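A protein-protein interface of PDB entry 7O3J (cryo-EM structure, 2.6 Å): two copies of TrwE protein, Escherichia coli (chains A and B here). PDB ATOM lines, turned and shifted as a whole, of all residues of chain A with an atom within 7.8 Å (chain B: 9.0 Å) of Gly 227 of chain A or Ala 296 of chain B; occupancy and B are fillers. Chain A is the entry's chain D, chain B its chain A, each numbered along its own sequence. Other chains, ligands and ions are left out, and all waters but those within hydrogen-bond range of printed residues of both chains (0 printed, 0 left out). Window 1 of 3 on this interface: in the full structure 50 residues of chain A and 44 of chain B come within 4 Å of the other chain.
The side-chain amide nitrogen (NE2) of Gln 225 of chain A sits at hydrogen-bond distance from the backbone carbonyl oxygen (O) of Arg 267 of chain B. O of Leu 293 of chain B sits at hydrogen-bond distance from N of Arg 220 of chain A (2.8 Å). The guanidinium group (NH1) of Arg 220 of chain A lies within salt-bridge range of the side-chain carboxylate (OE2) of Glu 295 of chain B (2.9 Å).
NE of Arg 267 of chain B is in hydrogen-bond range of O of Ala 296 of chain B (3.0 Å). The guanidinium group of Arg 267 of chain B sits at hydrogen-bond distance from the backbone carbonyl oxygen of Gly 297 of chain B (2.7 Å). The side-chain hydroxyl of Ser 287 of chain B sits at hydrogen-bond distance from the backbone NH of Ala 378 of chain B, 3.1 Å away. The backbone carbonyl oxygen of Pro 288 of chain B is in hydrogen-bond range of the backbone NH of Leu 376 of chain B (3.3 Å). N of Leu 293 of chain B lies close to OE1 of Glu 295 of chain B, 3.2 Å away. O of Val 222 of chain A sits at hydrogen-bond distance from OH of Tyr 257 of chain A, 2.9 Å away.
Thr 219 of chain A touches Leu 293 of chain B. CB of Thr 219 of chain A touches O of Gly 294 of chain B, at 3.9 Å. CG2 of Val 222 of chain A touches CB of Glu 295 of chain B, at 3.8 Å. Thr 224 of chain A touches Arg 267 of chain B. Gln 225 of chain A touches Ala 296 of chain B. Phe 269 of chain B touches Pro 226 of chain A. Pro 226 of chain A touches Ala 296 of chain B (O to CB, 3.9 Å). Gly 227 of chain A touches Ala 296 of chain B. Leu 376 of chain B touches Met 228 of chain A. Tyr 257 of chain A touches Ala 296 of chain B.
Of chain B, only Ala 296 (3.9 Å) comes within 4 Å of Gly 227 of chain A. Tyr 257 of chain A touches one residue of chain B. No residue of chain A comes within 4 Å of Gly 297 of chain B. Of the printed residues of chain A, Glu 295 of chain B touches Arg 220 and Val 222. Printed residues of chain A within 4 Å of Leu 376 of chain B: Met 228. Of the printed residues of chain A, Ala 266 of chain B touches Thr 224 (3.8 Å). Of the printed residues of chain B, Thr 224 of chain A touches Ala 266 and Arg 267. Of the printed residues of chain B, Val 222 of chain A touches Glu 295 (3.8 Å). The nearest residue of chain B that does not touch Gly 227 of chain A is Phe 269 of chain B (5.3 Å). The nearest printed residue of chain A that does not touch Leu 376 of chain B is Thr 219 of chain A (4.3 Å).
Hydrophobic or aromatic side chains of chain B that line the printed part of chain A: Phe 269, Ala 296, Leu 376 and Ala 378. Hydrophobic or aromatic side chains of chain A within 4 Å of the printed part of chain B: Val 222, Met 228 and Tyr 257.
Position printed for both chains: 270.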
ATOM      1  N   THR A 219      17.605 -25.028  -9.560  1.00  0.00           N
ATOM      2  CA  THR A 219      16.692 -24.503 -10.553  1.00  0.00           C
ATOM      3  C   THR A 219      16.521 -25.487 -11.701  1.00  0.00           C
ATOM      4  O   THR A 219      17.421 -26.254 -12.039  1.00  0.00           O
ATOM      5  CB  THR A 219      17.203 -23.170 -11.087  1.00  0.00           C
ATOM      6  OG1 THR A 219      18.492 -23.359 -11.675  1.00  0.00           O
ATOM      7  CG2 THR A 219      17.321 -22.170  -9.967  1.00  0.00           C
ATOM      8  N   ARG A 220      15.340 -25.462 -12.298  1.00  0.00           N
ATOM      9  CA  ARG A 220      15.089 -26.162 -13.546  1.00  0.00           C
ATOM     10  C   ARG A 220      15.628 -25.301 -14.676  1.00  0.00           C
ATOM     11  O   ARG A 220      15.457 -24.082 -14.660  1.00  0.00           O
ATOM     12  CB  ARG A 220      13.596 -26.422 -13.711  1.00  0.00           C
ATOM     13  CG  ARG A 220      13.166 -26.814 -15.085  1.00  0.00           C
ATOM     14  CD  ARG A 220      11.859 -27.550 -15.012  1.00  0.00           C
ATOM     15  NE  ARG A 220      11.463 -28.105 -16.296  1.00  0.00           N
ATOM     16  CZ  ARG A 220      10.511 -27.594 -17.065  1.00  0.00           C
ATOM     17  NH1 ARG A 220       9.859 -26.511 -16.678  1.00  0.00           N
ATOM     18  NH2 ARG A 220      10.209 -28.166 -18.217  1.00  0.00           N
ATOM     19  N   LEU A 221      16.300 -25.917 -15.635  1.00  0.00           N
ATOM     20  CA  LEU A 221      17.056 -25.171 -16.629  1.00  0.00           C
ATOM     21  C   LEU A 221      16.394 -25.316 -17.996  1.00  0.00           C
ATOM     22  O   LEU A 221      16.225 -26.430 -18.491  1.00  0.00           O
ATOM     23  CB  LEU A 221      18.503 -25.657 -16.659  1.00  0.00           C
ATOM     24  CG  LEU A 221      19.568 -24.834 -17.377  1.00  0.00           C
ATOM     25  CD1 LEU A 221      20.897 -25.106 -16.741  1.00  0.00           C
ATOM     26  CD2 LEU A 221      19.638 -25.168 -18.826  1.00  0.00           C
ATOM     27  N   VAL A 222      16.017 -24.188 -18.592  1.00  0.00           N
ATOM     28  CA  VAL A 222      15.448 -24.129 -19.934  1.00  0.00           C
ATOM     29  C   VAL A 222      16.173 -23.018 -20.675  1.00  0.00           C
ATOM     30  O   VAL A 222      16.162 -21.869 -20.227  1.00  0.00           O
ATOM     31  CB  VAL A 222      13.934 -23.868 -19.912  1.00  0.00           C
ATOM     32  CG1 VAL A 222      13.394 -23.778 -21.310  1.00  0.00           C
ATOM     33  CG2 VAL A 222      13.218 -24.953 -19.144  1.00  0.00           C
ATOM     34  N   THR A 223      16.792 -23.347 -21.806  1.00  0.00           N
ATOM     35  CA  THR A 223      17.732 -22.435 -22.441  1.00  0.00           C
ATOM     36  C   THR A 223      17.092 -21.511 -23.461  1.00  0.00           C
ATOM     37  O   THR A 223      17.795 -21.012 -24.343  1.00  0.00           O
ATOM     38  CB  THR A 223      18.864 -23.209 -23.113  1.00  0.00           C
ATOM     39  OG1 THR A 223      18.361 -23.894 -24.262  1.00  0.00           O
ATOM     40  CG2 THR A 223      19.458 -24.196 -22.164  1.00  0.00           C
ATOM     41  N   THR A 224      15.790 -21.257 -23.369  1.00  0.00           N
ATOM     42  CA  THR A 224      15.174 -20.300 -24.282  1.00  0.00           C
ATOM     43  C   THR A 224      15.778 -18.913 -24.109  1.00  0.00           C
ATOM     44  O   THR A 224      16.209 -18.283 -25.080  1.00  0.00           O
ATOM     45  CB  THR A 224      13.667 -20.254 -24.062  1.00  0.00           C
ATOM     46  OG1 THR A 224      13.139 -21.582 -24.082  1.00  0.00           O
ATOM     47  CG2 THR A 224      13.007 -19.445 -25.145  1.00  0.00           C
ATOM     48  N   GLN A 225      15.828 -18.426 -22.875  1.00  0.00           N
ATOM     49  CA  GLN A 225      16.345 -17.121 -22.523  1.00  0.00           C
ATOM     50  C   GLN A 225      17.612 -17.261 -21.693  1.00  0.00           C
ATOM     51  O   GLN A 225      17.765 -18.239 -20.960  1.00  0.00           O
ATOM     52  CB  GLN A 225      15.319 -16.313 -21.723  1.00  0.00           C
ATOM     53  CG  GLN A 225      14.007 -16.077 -22.416  1.00  0.00           C
ATOM     54  CD  GLN A 225      14.124 -15.145 -23.592  1.00  0.00           C
ATOM     55  OE1 GLN A 225      15.029 -14.325 -23.660  1.00  0.00           O
ATOM     56  NE2 GLN A 225      13.193 -15.252 -24.521  1.00  0.00           N
ATOM     57  N   PRO A 226      18.539 -16.311 -21.784  1.00  0.00           N
ATOM     58  CA  PRO A 226      19.690 -16.327 -20.880  1.00  0.00           C
ATOM     59  C   PRO A 226      19.229 -16.176 -19.445  1.00  0.00           C
ATOM     60  O   PRO A 226      18.257 -15.481 -19.157  1.00  0.00           O
ATOM     61  CB  PRO A 226      20.513 -15.125 -21.339  1.00  0.00           C
ATOM     62  CG  PRO A 226      19.539 -14.237 -21.975  1.00  0.00           C
ATOM     63  CD  PRO A 226      18.553 -15.125 -22.652  1.00  0.00           C
ATOM     64  N   GLY A 227      19.924 -16.838 -18.535  1.00  0.00           N
ATOM     65  CA  GLY A 227      19.462 -16.831 -17.167  1.00  0.00           C
ATOM     66  C   GLY A 227      20.551 -17.257 -16.216  1.00  0.00           C
ATOM     67  O   GLY A 227      21.691 -17.496 -16.608  1.00  0.00           O
ATOM     68  N   MET A 228      20.180 -17.345 -14.948  1.00  0.00           N
ATOM     69  CA  MET A 228      21.092 -17.708 -13.882  1.00  0.00           C
ATOM     70  C   MET A 228      20.678 -19.030 -13.265  1.00  0.00           C
ATOM     71  O   MET A 228      19.491 -19.290 -13.067  1.00  0.00           O
ATOM     72  CB  MET A 228      21.134 -16.627 -12.812  1.00  0.00           C
ATOM     73  CG  MET A 228      21.748 -15.358 -13.307  1.00  0.00           C
ATOM     74  SD  MET A 228      21.803 -14.073 -12.073  1.00  0.00           S
ATOM     75  CE  MET A 228      22.490 -12.768 -13.067  1.00  0.00           C
ATOM     76  N   THR A 229      21.664 -19.859 -12.969  1.00  0.00           N
ATOM     77  CA  THR A 229      21.455 -21.153 -12.354  1.00  0.00           C
ATOM     78  C   THR A 229      21.862 -21.080 -10.893  1.00  0.00           C
ATOM     79  O   THR A 229      22.447 -20.097 -10.440  1.00  0.00           O
ATOM     80  CB  THR A 229      22.258 -22.241 -13.071  1.00  0.00           C
ATOM     81  OG1 THR A 229      23.624 -21.835 -13.167  1.00  0.00           O
ATOM     82  CG2 THR A 229      21.737 -22.442 -14.464  1.00  0.00           C
ATOM     83  N   GLY A 255      25.540 -19.429 -10.850  1.00  0.00           N
ATOM     84  CA  GLY A 255      26.152 -19.379 -12.157  1.00  0.00           C
ATOM     85  C   GLY A 255      25.219 -18.802 -13.190  1.00  0.00           C
ATOM     86  O   GLY A 255      24.158 -18.292 -12.842  1.00  0.00           O
ATOM     87  N   PHE A 256      25.594 -18.868 -14.460  1.00  0.00           N
ATOM     88  CA  PHE A 256      24.728 -18.359 -15.508  1.00  0.00           C
ATOM     89  C   PHE A 256      25.106 -19.003 -16.829  1.00  0.00           C
ATOM     90  O   PHE A 256      26.204 -19.532 -16.992  1.00  0.00           O
ATOM     91  CB  PHE A 256      24.800 -16.833 -15.603  1.00  0.00           C
ATOM     92  CG  PHE A 256      26.079 -16.323 -16.182  1.00  0.00           C
ATOM     93  CD1 PHE A 256      27.204 -16.208 -15.399  1.00  0.00           C
ATOM     94  CD2 PHE A 256      26.152 -15.947 -17.504  1.00  0.00           C
ATOM     95  CE1 PHE A 256      28.371 -15.744 -15.926  1.00  0.00           C
ATOM     96  CE2 PHE A 256      27.318 -15.484 -18.032  1.00  0.00           C
ATOM     97  CZ  PHE A 256      28.430 -15.380 -17.242  1.00  0.00           C
ATOM     98  N   TYR A 257      24.174 -18.947 -17.770  1.00  0.00           N
ATOM     99  CA  TYR A 257      24.386 -19.420 -19.126  1.00  0.00           C
ATOM    100  C   TYR A 257      23.839 -18.372 -20.076  1.00  0.00           C
ATOM    101  O   TYR A 257      23.090 -17.481 -19.682  1.00  0.00           O
ATOM    102  CB  TYR A 257      23.711 -20.772 -19.359  1.00  0.00           C
ATOM    103  CG  TYR A 257      22.228 -20.729 -19.137  1.00  0.00           C
ATOM    104  CD1 TYR A 257      21.694 -20.920 -17.880  1.00  0.00           C
ATOM    105  CD2 TYR A 257      21.362 -20.480 -20.185  1.00  0.00           C
ATOM    106  CE1 TYR A 257      20.348 -20.866 -17.676  1.00  0.00           C
ATOM    107  CE2 TYR A 257      20.018 -20.424 -19.987  1.00  0.00           C
ATOM    108  CZ  TYR A 257      19.515 -20.617 -18.732  1.00  0.00           C
ATOM    109  OH  TYR A 257      18.162 -20.567 -18.533  1.00  0.00           O
ATOM    110  N   GLN A 258      24.225 -18.473 -21.341  1.00  0.00           N
ATOM    111  CA  GLN A 258      23.717 -17.563 -22.357  1.00  0.00           C
ATOM    112  C   GLN A 258      24.023 -18.145 -23.725  1.00  0.00           C
ATOM    113  O   GLN A 258      24.786 -19.104 -23.857  1.00  0.00           O
ATOM    114  CB  GLN A 258      24.329 -16.176 -22.224  1.00  0.00           C
ATOM    115  CG  GLN A 258      25.810 -16.170 -22.415  1.00  0.00           C
ATOM    116  CD  GLN A 258      26.426 -14.879 -21.989  1.00  0.00           C
ATOM    117  OE1 GLN A 258      25.763 -14.033 -21.405  1.00  0.00           O
ATOM    118  NE2 GLN A 258      27.704 -14.714 -22.272  1.00  0.00           N
ATOM    119  N   GLY A 259      23.408 -17.555 -24.743  1.00  0.00           N
ATOM    120  CA  GLY A 259      23.718 -17.855 -26.119  1.00  0.00           C
ATOM    121  C   GLY A 259      22.885 -18.946 -26.749  1.00  0.00           C
ATOM    122  O   GLY A 259      22.814 -19.016 -27.977  1.00  0.00           O
ATOM    123  N   VAL A 270      27.719 -23.643 -19.050  1.00  0.00           N
ATOM    124  CA  VAL A 270      27.335 -22.954 -17.828  1.00  0.00           C
ATOM    125  C   VAL A 270      28.602 -22.547 -17.101  1.00  0.00           C
ATOM    126  O   VAL A 270      29.499 -23.370 -16.904  1.00  0.00           O
ATOM    127  CB  VAL A 270      26.454 -23.834 -16.926  1.00  0.00           C
ATOM    128  CG1 VAL A 270      26.149 -23.121 -15.633  1.00  0.00           C
ATOM    129  CG2 VAL A 270      25.178 -24.193 -17.637  1.00  0.00           C
ATOM    130  N   GLN A 271      28.680 -21.282 -16.719  1.00  0.00           N
ATOM    131  CA  GLN A 271      29.775 -20.765 -15.916  1.00  0.00           C
ATOM    132  C   GLN A 271      29.288 -20.533 -14.500  1.00  0.00           C
ATOM    133  O   GLN A 271      28.362 -19.752 -14.284  1.00  0.00           O
ATOM    134  CB  GLN A 271      30.312 -19.463 -16.491  1.00  0.00           C
ATOM    135  CG  GLN A 271      31.266 -18.795 -15.557  1.00  0.00           C
ATOM    136  CD  GLN A 271      31.711 -17.459 -16.044  1.00  0.00           C
ATOM    137  OE1 GLN A 271      32.395 -16.736 -15.337  1.00  0.00           O
ATOM    138  NE2 GLN A 271      31.337 -17.119 -17.261  1.00  0.00           N
ATOM    139  N   ALA B 266       9.385 -19.773 -26.357  1.00  0.00           N
ATOM    140  CA  ALA B 266       8.157 -19.866 -25.583  1.00  0.00           C
ATOM    141  C   ALA B 266       8.256 -19.163 -24.238  1.00  0.00           C
ATOM    142  O   ALA B 266       7.357 -19.317 -23.408  1.00  0.00           O
ATOM    143  CB  ALA B 266       7.773 -21.330 -25.377  1.00  0.00           C
ATOM    144  N   ARG B 267       9.324 -18.410 -23.997  1.00  0.00           N
ATOM    145  CA  ARG B 267       9.529 -17.712 -22.738  1.00  0.00           C
ATOM    146  C   ARG B 267      10.079 -16.326 -23.022  1.00  0.00           C
ATOM    147  O   ARG B 267      10.926 -16.159 -23.898  1.00  0.00           O
ATOM    148  CB  ARG B 267      10.483 -18.483 -21.830  1.00  0.00           C
ATOM    149  CG  ARG B 267      10.031 -19.886 -21.522  1.00  0.00           C
ATOM    150  CD  ARG B 267      10.853 -20.504 -20.433  1.00  0.00           C
ATOM    151  NE  ARG B 267      10.452 -20.023 -19.124  1.00  0.00           N
ATOM    152  CZ  ARG B 267       9.493 -20.569 -18.393  1.00  0.00           C
ATOM    153  NH1 ARG B 267       8.840 -21.623 -18.842  1.00  0.00           N
ATOM    154  NH2 ARG B 267       9.190 -20.062 -17.214  1.00  0.00           N
ATOM    155  N   ILE B 268       9.590 -15.340 -22.281  1.00  0.00           N
ATOM    156  CA  ILE B 268       9.989 -13.946 -22.434  1.00  0.00           C
ATOM    157  C   ILE B 268      10.897 -13.575 -21.274  1.00  0.00           C
ATOM    158  O   ILE B 268      10.708 -14.050 -20.153  1.00  0.00           O
ATOM    159  CB  ILE B 268       8.755 -13.022 -22.507  1.00  0.00           C
ATOM    160  CG1 ILE B 268       9.145 -11.596 -22.880  1.00  0.00           C
ATOM    161  CG2 ILE B 268       7.998 -13.012 -21.203  1.00  0.00           C
ATOM    162  CD1 ILE B 268       9.594 -11.433 -24.284  1.00  0.00           C
ATOM    163  N   PHE B 269      11.900 -12.749 -21.540  1.00  0.00           N
ATOM    164  CA  PHE B 269      12.790 -12.283 -20.488  1.00  0.00           C
ATOM    165  C   PHE B 269      12.142 -11.112 -19.763  1.00  0.00           C
ATOM    166  O   PHE B 269      11.780 -10.111 -20.388  1.00  0.00           O
ATOM    167  CB  PHE B 269      14.143 -11.873 -21.062  1.00  0.00           C
ATOM    168  CG  PHE B 269      15.185 -11.609 -20.019  1.00  0.00           C
ATOM    169  CD1 PHE B 269      16.020 -12.614 -19.591  1.00  0.00           C
ATOM    170  CD2 PHE B 269      15.322 -10.357 -19.460  1.00  0.00           C
ATOM    171  CE1 PHE B 269      16.966 -12.371 -18.631  1.00  0.00           C
ATOM    172  CE2 PHE B 269      16.261 -10.118 -18.499  1.00  0.00           C
ATOM    173  CZ  PHE B 269      17.084 -11.123 -18.086  1.00  0.00           C
ATOM    174  N   VAL B 270      12.006 -11.232 -18.448  1.00  0.00           N
ATOM    175  CA  VAL B 270      11.456 -10.182 -17.605  1.00  0.00           C
ATOM    176  C   VAL B 270      12.524  -9.773 -16.609  1.00  0.00           C
ATOM    177  O   VAL B 270      13.124 -10.628 -15.951  1.00  0.00           O
ATOM    178  CB  VAL B 270      10.183 -10.642 -16.873  1.00  0.00           C
ATOM    179  CG1 VAL B 270       9.694  -9.562 -15.942  1.00  0.00           C
ATOM    180  CG2 VAL B 270       9.114 -10.999 -17.867  1.00  0.00           C
ATOM    181  N   SER B 287      17.026  -7.853 -11.451  1.00  0.00           N
ATOM    182  CA  SER B 287      17.218  -9.283 -11.410  1.00  0.00           C
ATOM    183  C   SER B 287      16.343  -9.972 -12.442  1.00  0.00           C
ATOM    184  O   SER B 287      15.308  -9.436 -12.840  1.00  0.00           O
ATOM    185  CB  SER B 287      16.880  -9.827 -10.020  1.00  0.00           C
ATOM    186  OG  SER B 287      17.749  -9.282  -9.051  1.00  0.00           O
ATOM    187  N   PRO B 288      16.735 -11.154 -12.901  1.00  0.00           N
ATOM    188  CA  PRO B 288      15.916 -11.870 -13.876  1.00  0.00           C
ATOM    189  C   PRO B 288      14.716 -12.544 -13.232  1.00  0.00           C
ATOM    190  O   PRO B 288      14.807 -13.137 -12.157  1.00  0.00           O
ATOM    191  CB  PRO B 288      16.892 -12.899 -14.450  1.00  0.00           C
ATOM    192  CG  PRO B 288      17.833 -13.135 -13.358  1.00  0.00           C
ATOM    193  CD  PRO B 288      18.022 -11.828 -12.683  1.00  0.00           C
ATOM    194  N   GLY B 289      13.577 -12.443 -13.908  1.00  0.00           N
ATOM    195  CA  GLY B 289      12.386 -13.154 -13.495  1.00  0.00           C
ATOM    196  C   GLY B 289      12.358 -14.543 -14.105  1.00  0.00           C
ATOM    197  O   GLY B 289      12.790 -14.749 -15.235  1.00  0.00           O
ATOM    198  N   THR B 290      11.843 -15.494 -13.340  1.00  0.00           N
ATOM    199  CA  THR B 290      11.892 -16.899 -13.701  1.00  0.00           C
ATOM    200  C   THR B 290      10.523 -17.524 -13.475  1.00  0.00           C
ATOM    201  O   THR B 290       9.566 -16.854 -13.087  1.00  0.00           O
ATOM    202  CB  THR B 290      12.975 -17.628 -12.894  1.00  0.00           C
ATOM    203  OG1 THR B 290      12.755 -17.422 -11.496  1.00  0.00           O
ATOM    204  CG2 THR B 290      14.351 -17.104 -13.243  1.00  0.00           C
ATOM    205  N   GLY B 291      10.425 -18.819 -13.736  1.00  0.00           N
ATOM    206  CA  GLY B 291       9.224 -19.552 -13.436  1.00  0.00           C
ATOM    207  C   GLY B 291       9.205 -20.023 -12.006  1.00  0.00           C
ATOM    208  O   GLY B 291      10.087 -19.716 -11.202  1.00  0.00           O
ATOM    209  N   PRO B 292       8.171 -20.790 -11.665  1.00  0.00           N
ATOM    210  CA  PRO B 292       8.068 -21.300 -10.290  1.00  0.00           C
ATOM    211  C   PRO B 292       9.226 -22.189  -9.882  1.00  0.00           C
ATOM    212  O   PRO B 292       9.545 -22.262  -8.692  1.00  0.00           O
ATOM    213  CB  PRO B 292       6.744 -22.071 -10.306  1.00  0.00           C
ATOM    214  CG  PRO B 292       6.007 -21.537 -11.453  1.00  0.00           C
ATOM    215  CD  PRO B 292       7.018 -21.184 -12.479  1.00  0.00           C
ATOM    216  N   LEU B 293       9.864 -22.876 -10.828  1.00  0.00           N
ATOM    217  CA  LEU B 293      10.995 -23.742 -10.536  1.00  0.00           C
ATOM    218  C   LEU B 293      12.311 -23.160 -11.027  1.00  0.00           C
ATOM    219  O   LEU B 293      13.287 -23.894 -11.188  1.00  0.00           O
ATOM    220  CB  LEU B 293      10.779 -25.125 -11.137  1.00  0.00           C
ATOM    221  CG  LEU B 293       9.994 -26.090 -10.262  1.00  0.00           C
ATOM    222  CD1 LEU B 293       9.536 -27.249 -11.096  1.00  0.00           C
ATOM    223  CD2 LEU B 293      10.838 -26.558  -9.108  1.00  0.00           C
ATOM    224  N   GLY B 294      12.357 -21.860 -11.274  1.00  0.00           N
ATOM    225  CA  GLY B 294      13.596 -21.190 -11.578  1.00  0.00           C
ATOM    226  C   GLY B 294      14.030 -21.216 -13.021  1.00  0.00           C
ATOM    227  O   GLY B 294      15.142 -20.773 -13.317  1.00  0.00           O
ATOM    228  N   GLU B 295      13.205 -21.722 -13.927  1.00  0.00           N
ATOM    229  CA  GLU B 295      13.560 -21.693 -15.336  1.00  0.00           C
ATOM    230  C   GLU B 295      13.432 -20.282 -15.895  1.00  0.00           C
ATOM    231  O   GLU B 295      12.502 -19.548 -15.564  1.00  0.00           O
ATOM    232  CB  GLU B 295      12.712 -22.698 -16.110  1.00  0.00           C
ATOM    233  CG  GLU B 295      11.251 -22.413 -16.115  1.00  0.00           C
ATOM    234  CD  GLU B 295      10.527 -23.159 -15.016  1.00  0.00           C
ATOM    235  OE1 GLU B 295      10.876 -22.959 -13.842  1.00  0.00           O
ATOM    236  OE2 GLU B 295       9.612 -23.946 -15.318  1.00  0.00           O
ATOM    237  N   ALA B 296      14.391 -19.904 -16.731  1.00  0.00           N
ATOM    238  CA  ALA B 296      14.591 -18.505 -17.075  1.00  0.00           C
ATOM    239  C   ALA B 296      13.449 -17.973 -17.919  1.00  0.00           C
ATOM    240  O   ALA B 296      13.036 -18.600 -18.895  1.00  0.00           O
ATOM    241  CB  ALA B 296      15.908 -18.331 -17.821  1.00  0.00           C
ATOM    242  N   GLY B 297      12.956 -16.801 -17.554  1.00  0.00           N
ATOM    243  CA  GLY B 297      11.900 -16.151 -18.290  1.00  0.00           C
ATOM    244  C   GLY B 297      10.520 -16.603 -17.852  1.00  0.00           C
ATOM    245  O   GLY B 297      10.337 -17.652 -17.243  1.00  0.00           O
ATOM    246  N   LEU B 298       9.535 -15.784 -18.178  1.00  0.00           N
ATOM    247  CA  LEU B 298       8.145 -16.130 -17.938  1.00  0.00           C
ATOM    248  C   LEU B 298       7.566 -16.799 -19.173  1.00  0.00           C
ATOM    249  O   LEU B 298       7.834 -16.384 -20.300  1.00  0.00           O
ATOM    250  CB  LEU B 298       7.333 -14.888 -17.579  1.00  0.00           C
ATOM    251  CG  LEU B 298       7.175 -14.567 -16.096  1.00  0.00           C
ATOM    252  CD1 LEU B 298       8.498 -14.278 -15.463  1.00  0.00           C
ATOM    253  CD2 LEU B 298       6.277 -13.372 -15.945  1.00  0.00           C
ATOM    254  N   GLY B 299       6.788 -17.843 -18.956  1.00  0.00           N
ATOM    255  CA  GLY B 299       6.190 -18.576 -20.052  1.00  0.00           C
ATOM    256  C   GLY B 299       4.731 -18.848 -19.777  1.00  0.00           C
ATOM    257  O   GLY B 299       4.318 -19.037 -18.634  1.00  0.00           O
ATOM    258  N   LEU B 365       2.974 -14.321 -26.477  1.00  0.00           N
ATOM    259  CA  LEU B 365       2.850 -15.058 -25.231  1.00  0.00           C
ATOM    260  C   LEU B 365       1.733 -14.470 -24.385  1.00  0.00           C
ATOM    261  O   LEU B 365       1.618 -13.254 -24.252  1.00  0.00           O
ATOM    262  CB  LEU B 365       4.161 -15.022 -24.453  1.00  0.00           C
ATOM    263  CG  LEU B 365       4.286 -15.875 -23.199  1.00  0.00           C
ATOM    264  CD1 LEU B 365       5.607 -16.553 -23.221  1.00  0.00           C
ATOM    265  CD2 LEU B 365       4.181 -15.009 -21.974  1.00  0.00           C
ATOM    266  N   ASN B 374       9.100 -16.572  -9.684  1.00  0.00           N
ATOM    267  CA  ASN B 374      10.250 -16.325  -8.828  1.00  0.00           C
ATOM    268  C   ASN B 374      11.081 -15.174  -9.364  1.00  0.00           C
ATOM    269  O   ASN B 374      11.122 -14.916 -10.567  1.00  0.00           O
ATOM    270  CB  ASN B 374      11.164 -17.546  -8.684  1.00  0.00           C
ATOM    271  CG  ASN B 374      10.547 -18.650  -7.874  1.00  0.00           C
ATOM    272  OD1 ASN B 374       9.915 -18.409  -6.849  1.00  0.00           O
ATOM    273  ND2 ASN B 374      10.736 -19.878  -8.317  1.00  0.00           N
ATOM    274  N   LEU B 376      15.043 -14.327  -9.055  1.00  0.00           N
ATOM    275  CA  LEU B 376      16.343 -14.818  -8.631  1.00  0.00           C
ATOM    276  C   LEU B 376      17.263 -13.619  -8.471  1.00  0.00           C
ATOM    277  O   LEU B 376      17.561 -12.928  -9.449  1.00  0.00           O
ATOM    278  CB  LEU B 376      16.892 -15.819  -9.644  1.00  0.00           C
ATOM    279  CG  LEU B 376      18.150 -16.620  -9.322  1.00  0.00           C
ATOM    280  CD1 LEU B 376      18.106 -17.929 -10.075  1.00  0.00           C
ATOM    281  CD2 LEU B 376      19.401 -15.862  -9.699  1.00  0.00           C
ATOM    282  N   ALA B 378      20.099 -11.267  -8.476  1.00  0.00           N
ATOM    283  CA  ALA B 378      21.306 -11.275  -9.287  1.00  0.00           C
ATOM    284  C   ALA B 378      22.477 -10.565  -8.634  1.00  0.00           C
ATOM    285  O   ALA B 378      23.600 -10.663  -9.137  1.00  0.00           O
ATOM    286  CB  ALA B 378      21.028 -10.627 -10.642  1.00  0.00           C
